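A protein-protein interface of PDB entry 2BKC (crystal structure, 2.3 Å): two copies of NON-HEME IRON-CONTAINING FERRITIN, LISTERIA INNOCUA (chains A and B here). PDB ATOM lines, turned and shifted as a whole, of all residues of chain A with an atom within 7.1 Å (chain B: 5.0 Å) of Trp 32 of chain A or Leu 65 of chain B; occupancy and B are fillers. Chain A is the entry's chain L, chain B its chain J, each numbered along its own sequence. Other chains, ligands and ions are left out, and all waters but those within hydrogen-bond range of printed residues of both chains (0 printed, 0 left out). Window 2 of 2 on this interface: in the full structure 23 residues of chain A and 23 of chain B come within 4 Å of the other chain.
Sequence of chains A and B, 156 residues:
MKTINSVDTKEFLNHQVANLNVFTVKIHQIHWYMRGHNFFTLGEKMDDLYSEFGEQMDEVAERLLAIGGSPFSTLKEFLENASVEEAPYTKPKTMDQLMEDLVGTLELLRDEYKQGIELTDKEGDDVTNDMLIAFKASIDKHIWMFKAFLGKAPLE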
ATOM      1  N   VAL A  25     -15.902  30.999  17.840  1.00  0.00           N
ATOM      2  CA  VAL A  25     -15.490  30.282  16.627  1.00  0.00           C
ATOM      3  C   VAL A  25     -16.585  29.304  16.166  1.00  0.00           C
ATOM      4  O   VAL A  25     -16.922  29.239  14.971  1.00  0.00           O
ATOM      5  CB  VAL A  25     -14.079  29.633  16.829  1.00  0.00           C
ATOM      6  CG1 VAL A  25     -13.725  28.652  15.680  1.00  0.00           C
ATOM      7  CG2 VAL A  25     -13.003  30.761  16.960  1.00  0.00           C
ATOM      8  N   LYS A  26     -17.216  28.632  17.114  1.00  0.00           N
ATOM      9  CA  LYS A  26     -18.361  27.780  16.796  1.00  0.00           C
ATOM     10  C   LYS A  26     -19.515  28.566  16.132  1.00  0.00           C
ATOM     11  O   LYS A  26     -20.165  28.057  15.227  1.00  0.00           O
ATOM     12  CB  LYS A  26     -18.821  27.052  18.038  1.00  0.00           C
ATOM     13  CG  LYS A  26     -19.862  25.922  17.839  1.00  0.00           C
ATOM     14  CD  LYS A  26     -20.487  25.502  19.208  1.00  0.00           C
ATOM     15  CE  LYS A  26     -19.899  24.202  19.788  1.00  0.00           C
ATOM     16  NZ  LYS A  26     -19.967  23.053  18.792  1.00  0.00           N
ATOM     17  N   ILE A  27     -19.755  29.805  16.531  1.00  0.00           N
ATOM     18  CA  ILE A  27     -20.847  30.559  15.916  1.00  0.00           C
ATOM     19  C   ILE A  27     -20.535  30.860  14.451  1.00  0.00           C
ATOM     20  O   ILE A  27     -21.402  30.757  13.591  1.00  0.00           O
ATOM     21  CB  ILE A  27     -21.165  31.862  16.689  1.00  0.00           C
ATOM     22  CG1 ILE A  27     -22.022  31.528  17.903  1.00  0.00           C
ATOM     23  CG2 ILE A  27     -21.907  32.866  15.769  1.00  0.00           C
ATOM     24  CD1 ILE A  27     -21.609  32.253  19.138  1.00  0.00           C
ATOM     25  N   HIS A  28     -19.304  31.228  14.155  1.00  0.00           N
ATOM     26  CA  HIS A  28     -18.896  31.361  12.756  1.00  0.00           C
ATOM     27  C   HIS A  28     -19.050  30.047  12.000  1.00  0.00           C
ATOM     28  O   HIS A  28     -19.450  30.063  10.849  1.00  0.00           O
ATOM     29  CB  HIS A  28     -17.442  31.802  12.660  1.00  0.00           C
ATOM     30  CG  HIS A  28     -17.243  33.287  12.696  1.00  0.00           C
ATOM     31  ND1 HIS A  28     -18.261  34.185  12.465  1.00  0.00           N
ATOM     32  CD2 HIS A  28     -16.130  34.026  12.911  1.00  0.00           C
ATOM     33  CE1 HIS A  28     -17.790  35.417  12.549  1.00  0.00           C
ATOM     34  NE2 HIS A  28     -16.498  35.350  12.818  1.00  0.00           N
ATOM     35  N   GLN A  29     -18.726  28.906  12.620  1.00  0.00           N
ATOM     36  CA  GLN A  29     -18.841  27.630  11.914  1.00  0.00           C
ATOM     37  C   GLN A  29     -20.294  27.440  11.458  1.00  0.00           C
ATOM     38  O   GLN A  29     -20.559  27.098  10.297  1.00  0.00           O
ATOM     39  CB  GLN A  29     -18.389  26.459  12.789  1.00  0.00           C
ATOM     40  CG  GLN A  29     -18.576  25.077  12.103  1.00  0.00           C
ATOM     41  CD  GLN A  29     -18.137  23.898  12.947  1.00  0.00           C
ATOM     42  OE1 GLN A  29     -16.956  23.528  12.946  1.00  0.00           O
ATOM     43  NE2 GLN A  29     -19.098  23.281  13.646  1.00  0.00           N
ATOM     44  N   ILE A  30     -21.231  27.700  12.370  1.00  0.00           N
ATOM     45  CA  ILE A  30     -22.650  27.547  12.082  1.00  0.00           C
ATOM     46  C   ILE A  30     -23.049  28.495  10.935  1.00  0.00           C
ATOM     47  O   ILE A  30     -23.698  28.094   9.986  1.00  0.00           O
ATOM     48  CB  ILE A  30     -23.471  27.821  13.340  1.00  0.00           C
ATOM     49  CG1 ILE A  30     -23.205  26.733  14.384  1.00  0.00           C
ATOM     50  CG2 ILE A  30     -24.986  27.831  13.011  1.00  0.00           C
ATOM     51  CD1 ILE A  30     -23.723  27.048  15.773  1.00  0.00           C
ATOM     52  N   HIS A  31     -22.606  29.745  11.030  1.00  0.00           N
ATOM     53  CA  HIS A  31     -22.930  30.763  10.042  1.00  0.00           C
ATOM     54  C   HIS A  31     -22.444  30.346   8.643  1.00  0.00           C
ATOM     55  O   HIS A  31     -23.225  30.315   7.674  1.00  0.00           O
ATOM     56  CB  HIS A  31     -22.341  32.124  10.444  1.00  0.00           C
ATOM     57  CG  HIS A  31     -22.885  33.270   9.650  1.00  0.00           C
ATOM     58  ND1 HIS A  31     -23.718  33.099   8.560  1.00  0.00           N
ATOM     59  CD2 HIS A  31     -22.704  34.604   9.773  1.00  0.00           C
ATOM     60  CE1 HIS A  31     -24.024  34.274   8.047  1.00  0.00           C
ATOM     61  NE2 HIS A  31     -23.416  35.205   8.760  1.00  0.00           N
ATOM     62  N   TRP A  32     -21.171  29.977   8.583  1.00  0.00           N
ATOM     63  CA  TRP A  32     -20.477  29.721   7.330  1.00  0.00           C
ATOM     64  C   TRP A  32     -21.033  28.526   6.577  1.00  0.00           C
ATOM     65  O   TRP A  32     -21.013  28.546   5.358  1.00  0.00           O
ATOM     66  CB  TRP A  32     -18.984  29.479   7.592  1.00  0.00           C
ATOM     67  CG  TRP A  32     -18.259  30.681   7.930  1.00  0.00           C
ATOM     68  CD1 TRP A  32     -18.636  31.940   7.682  1.00  0.00           C
ATOM     69  CD2 TRP A  32     -17.006  30.764   8.611  1.00  0.00           C
ATOM     70  NE1 TRP A  32     -17.697  32.823   8.152  1.00  0.00           N
ATOM     71  CE2 TRP A  32     -16.681  32.122   8.726  1.00  0.00           C
ATOM     72  CE3 TRP A  32     -16.115  29.821   9.135  1.00  0.00           C
ATOM     73  CZ2 TRP A  32     -15.521  32.572   9.361  1.00  0.00           C
ATOM     74  CZ3 TRP A  32     -14.930  30.269   9.729  1.00  0.00           C
ATOM     75  CH2 TRP A  32     -14.651  31.633   9.839  1.00  0.00           C
ATOM     76  N   TYR A  33     -21.529  27.521   7.314  1.00  0.00           N
ATOM     77  CA  TYR A  33     -21.876  26.210   6.773  1.00  0.00           C
ATOM     78  C   TYR A  33     -23.377  25.981   6.729  1.00  0.00           C
ATOM     79  O   TYR A  33     -23.847  24.968   6.212  1.00  0.00           O
ATOM     80  CB  TYR A  33     -21.222  25.078   7.598  1.00  0.00           C
ATOM     81  CG  TYR A  33     -19.747  24.869   7.294  1.00  0.00           C
ATOM     82  CD1 TYR A  33     -18.767  25.341   8.148  1.00  0.00           C
ATOM     83  CD2 TYR A  33     -19.342  24.215   6.129  1.00  0.00           C
ATOM     84  CE1 TYR A  33     -17.432  25.176   7.855  1.00  0.00           C
ATOM     85  CE2 TYR A  33     -18.019  24.031   5.829  1.00  0.00           C
ATOM     86  CZ  TYR A  33     -17.056  24.513   6.695  1.00  0.00           C
ATOM     87  OH  TYR A  33     -15.731  24.335   6.402  1.00  0.00           O
ATOM     88  N   MET A  34     -24.148  26.898   7.279  1.00  0.00           N
ATOM     89  CA  MET A  34     -25.583  26.640   7.400  1.00  0.00           C
ATOM     90  C   MET A  34     -26.233  26.665   6.020  1.00  0.00           C
ATOM     91  O   MET A  34     -25.855  27.458   5.154  1.00  0.00           O
ATOM     92  CB  MET A  34     -26.271  27.636   8.336  1.00  0.00           C
ATOM     93  CG  MET A  34     -26.290  29.060   7.900  1.00  0.00           C
ATOM     94  SD  MET A  34     -27.355  30.212   8.949  1.00  0.00           S
ATOM     95  CE  MET A  34     -26.507  30.276  10.463  1.00  0.00           C
ATOM     96  N   ARG A  35     -27.206  25.795   5.832  1.00  0.00           N
ATOM     97  CA  ARG A  35     -28.028  25.828   4.636  1.00  0.00           C
ATOM     98  C   ARG A  35     -29.524  25.636   4.930  1.00  0.00           C
ATOM     99  O   ARG A  35     -29.881  25.224   6.030  1.00  0.00           O
ATOM    100  CB  ARG A  35     -27.540  24.726   3.717  1.00  0.00           C
ATOM    101  CG  ARG A  35     -26.097  24.839   3.332  1.00  0.00           C
ATOM    102  CD  ARG A  35     -25.809  23.902   2.210  1.00  0.00           C
ATOM    103  NE  ARG A  35     -24.427  23.903   1.748  1.00  0.00           N
ATOM    104  CZ  ARG A  35     -23.949  23.004   0.905  1.00  0.00           C
ATOM    105  NH1 ARG A  35     -24.754  22.060   0.424  1.00  0.00           N
ATOM    106  NH2 ARG A  35     -22.677  23.044   0.523  1.00  0.00           N
ATOM    107  N   PHE A  39     -31.684  30.414   6.046  1.00  0.00           N
ATOM    108  CA  PHE A  39     -30.296  30.830   5.970  1.00  0.00           C
ATOM    109  C   PHE A  39     -30.167  32.313   6.271  1.00  0.00           C
ATOM    110  O   PHE A  39     -29.244  32.707   6.976  1.00  0.00           O
ATOM    111  CB  PHE A  39     -29.683  30.446   4.609  1.00  0.00           C
ATOM    112  CG  PHE A  39     -28.352  31.100   4.323  1.00  0.00           C
ATOM    113  CD1 PHE A  39     -27.164  30.434   4.585  1.00  0.00           C
ATOM    114  CD2 PHE A  39     -28.296  32.365   3.773  1.00  0.00           C
ATOM    115  CE1 PHE A  39     -25.950  31.033   4.322  1.00  0.00           C
ATOM    116  CE2 PHE A  39     -27.082  32.972   3.503  1.00  0.00           C
ATOM    117  CZ  PHE A  39     -25.919  32.319   3.764  1.00  0.00           C
ATOM    118  N   MET A  46     -26.842  34.728  13.769  1.00  0.00           N
ATOM    119  CA  MET A  46     -25.457  34.347  14.117  1.00  0.00           C
ATOM    120  C   MET A  46     -24.524  35.529  14.186  1.00  0.00           C
ATOM    121  O   MET A  46     -23.649  35.513  15.052  1.00  0.00           O
ATOM    122  CB  MET A  46     -24.853  33.259  13.196  1.00  0.00           C
ATOM    123  CG  MET A  46     -25.470  31.873  13.303  1.00  0.00           C
ATOM    124  SD  MET A  46     -25.652  31.210  14.999  1.00  0.00           S
ATOM    125  CE  MET A  46     -27.216  31.721  15.328  1.00  0.00           C
ATOM    126  N   VAL B  17      -7.381  31.969   6.776  1.00  0.00           N
ATOM    127  CA  VAL B  17      -8.368  31.853   7.822  1.00  0.00           C
ATOM    128  C   VAL B  17      -7.729  31.480   9.167  1.00  0.00           C
ATOM    129  O   VAL B  17      -8.026  32.106  10.192  1.00  0.00           O
ATOM    130  CB  VAL B  17      -9.476  30.856   7.530  1.00  0.00           C
ATOM    131  CG1 VAL B  17     -10.372  30.699   8.777  1.00  0.00           C
ATOM    132  CG2 VAL B  17     -10.321  31.330   6.415  1.00  0.00           C
ATOM    133  N   MET B  57     -10.914  38.465   8.093  1.00  0.00           N
ATOM    134  CA  MET B  57     -11.078  37.032   8.255  1.00  0.00           C
ATOM    135  C   MET B  57     -12.440  36.531   7.752  1.00  0.00           C
ATOM    136  O   MET B  57     -12.503  35.557   7.033  1.00  0.00           O
ATOM    137  CB  MET B  57     -10.886  36.701   9.749  1.00  0.00           C
ATOM    138  CG  MET B  57     -10.720  35.242  10.061  1.00  0.00           C
ATOM    139  SD  MET B  57     -12.284  34.450  10.281  1.00  0.00           S
ATOM    140  CE  MET B  57     -12.711  35.086  11.977  1.00  0.00           C
ATOM    141  N   ASP B  58     -13.525  37.212   8.098  1.00  0.00           N
ATOM    142  CA  ASP B  58     -14.845  36.852   7.540  1.00  0.00           C
ATOM    143  C   ASP B  58     -14.843  36.890   6.026  1.00  0.00           C
ATOM    144  O   ASP B  58     -15.532  36.096   5.389  1.00  0.00           O
ATOM    145  CB  ASP B  58     -15.924  37.876   7.963  1.00  0.00           C
ATOM    146  CG  ASP B  58     -16.121  37.976   9.477  1.00  0.00           C
ATOM    147  OD1 ASP B  58     -16.913  38.840   9.894  1.00  0.00           O
ATOM    148  OD2 ASP B  58     -15.575  37.243  10.316  1.00  0.00           O
ATOM    149  N   ALA B  61     -13.027  34.062   4.578  1.00  0.00           N
ATOM    150  CA  ALA B  61     -13.819  32.853   4.697  1.00  0.00           C
ATOM    151  C   ALA B  61     -14.989  32.779   3.740  1.00  0.00           C
ATOM    152  O   ALA B  61     -15.225  31.712   3.172  1.00  0.00           O
ATOM    153  CB  ALA B  61     -14.328  32.681   6.121  1.00  0.00           C
ATOM    154  N   GLU B  62     -15.730  33.896   3.607  1.00  0.00           N
ATOM    155  CA  GLU B  62     -16.833  34.057   2.656  1.00  0.00           C
ATOM    156  C   GLU B  62     -16.384  33.970   1.181  1.00  0.00           C
ATOM    157  O   GLU B  62     -17.110  33.423   0.322  1.00  0.00           O
ATOM    158  CB  GLU B  62     -17.556  35.405   2.878  1.00  0.00           C
ATOM    159  CG  GLU B  62     -18.299  35.435   4.207  1.00  0.00           C
ATOM    160  CD  GLU B  62     -19.044  36.736   4.515  1.00  0.00           C
ATOM    161  OE1 GLU B  62     -19.059  37.681   3.689  1.00  0.00           O
ATOM    162  OE2 GLU B  62     -19.644  36.780   5.618  1.00  0.00           O
ATOM    163  N   ARG B  63     -15.211  34.521   0.880  1.00  0.00           N
ATOM    164  CA  ARG B  63     -14.672  34.371  -0.465  1.00  0.00           C
ATOM    165  C   ARG B  63     -14.380  32.877  -0.693  1.00  0.00           C
ATOM    166  O   ARG B  63     -14.804  32.316  -1.685  1.00  0.00           O
ATOM    167  CB  ARG B  63     -13.446  35.258  -0.722  1.00  0.00           C
ATOM    168  CG  ARG B  63     -12.964  35.279  -2.189  1.00  0.00           C
ATOM    169  CD  ARG B  63     -14.031  35.681  -3.241  1.00  0.00           C
ATOM    170  NE  ARG B  63     -13.563  35.372  -4.597  1.00  0.00           N
ATOM    171  CZ  ARG B  63     -14.344  35.031  -5.633  1.00  0.00           C
ATOM    172  NH1 ARG B  63     -15.658  35.009  -5.536  1.00  0.00           N
ATOM    173  NH2 ARG B  63     -13.793  34.720  -6.791  1.00  0.00           N
ATOM    174  N   LEU B  64     -13.736  32.219   0.264  1.00  0.00           N
ATOM    175  CA  LEU B  64     -13.504  30.777   0.162  1.00  0.00           C
ATOM    176  C   LEU B  64     -14.813  30.044  -0.075  1.00  0.00           C
ATOM    177  O   LEU B  64     -14.904  29.245  -0.994  1.00  0.00           O
ATOM    178  CB  LEU B  64     -12.783  30.269   1.397  1.00  0.00           C
ATOM    179  CG  LEU B  64     -12.371  28.797   1.449  1.00  0.00           C
ATOM    180  CD1 LEU B  64     -11.555  28.374   0.249  1.00  0.00           C
ATOM    181  CD2 LEU B  64     -11.602  28.564   2.718  1.00  0.00           C
ATOM    182  N   LEU B  65     -15.867  30.382   0.667  1.00  0.00           N
ATOM    183  CA  LEU B  65     -17.170  29.733   0.473  1.00  0.00           C
ATOM    184  C   LEU B  65     -17.636  29.963  -0.969  1.00  0.00           C
ATOM    185  O   LEU B  65     -18.115  29.055  -1.629  1.00  0.00           O
ATOM    186  CB  LEU B  65     -18.216  30.282   1.452  1.00  0.00           C
ATOM    187  CG  LEU B  65     -18.570  29.651   2.824  1.00  0.00           C
ATOM    188  CD1 LEU B  65     -18.211  28.166   2.951  1.00  0.00           C
ATOM    189  CD2 LEU B  65     -18.038  30.423   4.019  1.00  0.00           C
ATOM    190  N   ALA B  66     -17.484  31.194  -1.448  1.00  0.00           N
ATOM    191  CA  ALA B  66     -18.008  31.609  -2.750  1.00  0.00           C
ATOM    192  C   ALA B  66     -17.385  30.817  -3.931  1.00  0.00           C
ATOM    193  O   ALA B  66     -18.016  30.661  -4.989  1.00  0.00           O
ATOM    194  CB  ALA B  66     -17.816  33.142  -2.939  1.00  0.00           C
ATOM    195  N   ILE B  67     -16.177  30.291  -3.720  1.00  0.00           N
ATOM    196  CA  ILE B  67     -15.484  29.514  -4.746  1.00  0.00           C
ATOM    197  C   ILE B  67     -15.500  28.018  -4.508  1.00  0.00           C
ATOM    198  O   ILE B  67     -14.712  27.280  -5.132  1.00  0.00           O
ATOM    199  CB  ILE B  67     -14.022  29.989  -4.941  1.00  0.00           C
ATOM    200  CG1 ILE B  67     -13.155  29.654  -3.728  1.00  0.00           C
ATOM    201  CG2 ILE B  67     -13.980  31.476  -5.295  1.00  0.00           C
ATOM    202  CD1 ILE B  67     -11.690  30.164  -3.860  1.00  0.00           C
ATOM    203  N   GLY B  68     -16.395  27.552  -3.628  1.00  0.00           N
ATOM    204  CA  GLY B  68     -16.571  26.127  -3.437  1.00  0.00           C
ATOM    205  C   GLY B  68     -15.743  25.500  -2.337  1.00  0.00           C
ATOM    206  O   GLY B  68     -15.657  24.290  -2.238  1.00  0.00           O
ATOM    207  N   GLY B  69     -15.198  26.336  -1.465  1.00  0.00           N
ATOM    208  CA  GLY B  69     -14.307  25.894  -0.415  1.00  0.00           C
ATOM    209  C   GLY B  69     -15.059  25.603   0.868  1.00  0.00           C
ATOM    210  O   GLY B  69     -16.269  25.865   0.967  1.00  0.00           O
ATOM    211  N   SER B  70     -14.294  25.074   1.817  1.00  0.00           N
ATOM    212  CA  SER B  70     -14.699  24.732   3.174  1.00  0.00           C
ATOM    213  C   SER B  70     -13.749  25.347   4.232  1.00  0.00           C
ATOM    214  O   SER B  70     -12.707  24.809   4.535  1.00  0.00           O
ATOM    215  CB  SER B  70     -14.711  23.202   3.323  1.00  0.00           C
ATOM    216  OG  SER B  70     -15.633  22.651   2.395  1.00  0.00           O
ATOM    217  N   PRO B  71     -14.122  26.458   4.833  1.00  0.00           N
ATOM    218  CA  PRO B  71     -13.250  27.102   5.832  1.00  0.00           C
ATOM    219  C   PRO B  71     -12.929  26.240   7.040  1.00  0.00           C
ATOM    220  O   PRO B  71     -13.799  25.585   7.573  1.00  0.00           O
ATOM    221  CB  PRO B  71     -14.052  28.312   6.297  1.00  0.00           C
ATOM    222  CG  PRO B  71     -15.213  28.434   5.373  1.00  0.00           C
ATOM    223  CD  PRO B  71     -15.372  27.185   4.613  1.00  0.00           C
ATOM    224  N   PHE B  72     -11.667  26.256   7.469  1.00  0.00           N
ATOM    225  CA  PHE B  72     -11.299  25.808   8.817  1.00  0.00           C
ATOM    226  C   PHE B  72     -12.246  26.532   9.817  1.00  0.00           C
ATOM    227  O   PHE B  72     -12.474  27.746   9.703  1.00  0.00           O
ATOM    228  CB  PHE B  72      -9.824  26.154   9.130  1.00  0.00           C
ATOM    229  CG  PHE B  72      -8.790  25.463   8.240  1.00  0.00           C
ATOM    230  CD1 PHE B  72      -7.684  26.189   7.751  1.00  0.00           C
ATOM    231  CD2 PHE B  72      -8.887  24.102   7.922  1.00  0.00           C
ATOM    232  CE1 PHE B  72      -6.705  25.587   6.950  1.00  0.00           C
ATOM    233  CE2 PHE B  72      -7.916  23.484   7.112  1.00  0.00           C
ATOM    234  CZ  PHE B  72      -6.820  24.233   6.627  1.00  0.00           C
ATOM    235  N   SER B  73     -12.804  25.799  10.777  1.00  0.00           N
ATOM    236  CA  SER B  73     -13.786  26.366  11.682  1.00  0.00           C
ATOM    237  C   SER B  73     -13.694  25.841  13.119  1.00  0.00           C
ATOM    238  O   SER B  73     -14.718  25.761  13.828  1.00  0.00           O
ATOM    239  CB  SER B  73     -15.187  26.192  11.098  1.00  0.00           C
ATOM    240  OG  SER B  73     -15.615  24.851  11.050  1.00  0.00           O
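Ile 27 of chain A touches none of the printed residues of chain B.
Ile 30 of chain A touches none of the printed residues of chain B.
Of the printed residues of chain B, Trp 32 of chain A touches Met 57 (3.7 Å), Ala 61 (3.5 Å), Leu 65 (3.7 Å), Pro 71 (3.8 Å) and Phe 72 (3.5 Å).
Printed residues of chain A within 4 Å of Met 57 of chain B: His 28 (3.7 Å) and Trp 32 (3.7 Å).
Printed residues of chain A within 4 Å of Ala 61 of chain B: Trp 32 (3.5 Å).
Leu 65 of chain B touches just one residue of chain A: Trp 32 (3.7 Å).
Printed residues of chain A within 4 Å of Pro 71 of chain B: Trp 32 and Tyr 33.
The nearest printed residue of chain B that does not touch Trp 32 of chain A is Ser 73 of chain B (4.2 Å).
OD2 of Asp 58 of chain B lies within hydrogen-bond range of NE2 of His 28 of chain A.
The side-chain hydroxyl (OH) of Tyr 33 of chain A sits at hydrogen-bond distance from the backbone carbonyl oxygen (O) of Pro 71 of chain B (2.6 Å).
The side-chain hydroxyl (OG) of Ser 73 of chain B is in hydrogen-bond range of the side-chain amide oxygen (OE1) of Gln 29 of chain A, at 2.7 Å.
No position is printed for both chains.
Of the 16 printed residues of chain B, 8 touch a printed residue of chain A.
Hydrophobic or aromatic side chains of chain B within 4 Å of the printed part of chain A: Met 57, Ala 61, Leu 65 and Pro 71.
Along chain B the printed residues that touch a printed residue of chain A span positions 57 to 73.
Hydrophobic or aromatic side chains of chain A that line the printed part of chain B: Val 25, His 28, Trp 32 and Tyr 33.
O of Ser 73 of chain B touches CG1 of Val 25 of chain A, 3.6 Å away.
Met 57 of chain B touches His 28 of chain A.
CH2 of Trp 32 of chain A touches SD of Met 57 of chain B (3.7 Å).
CZ2 of Trp 32 of chain A touches CB of Ala 61 of chain B, at 3.5 Å.
O of Trp 32 of chain A touches CG of Leu 65 of chain B, 3.7 Å away.
Trp 32 of chain A touches Pro 71 of chain B (CE3 to CB, 3.8 Å).
Trp 32 of chain A touches Phe 72 of chain B.
OH of Tyr 33 of chain A touches C of Ser 70 of chain B, at 3.1 Å.
Tyr 33 of chain A touches Ser 73 of chain B (CE1 to OG, 3.7 Å).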
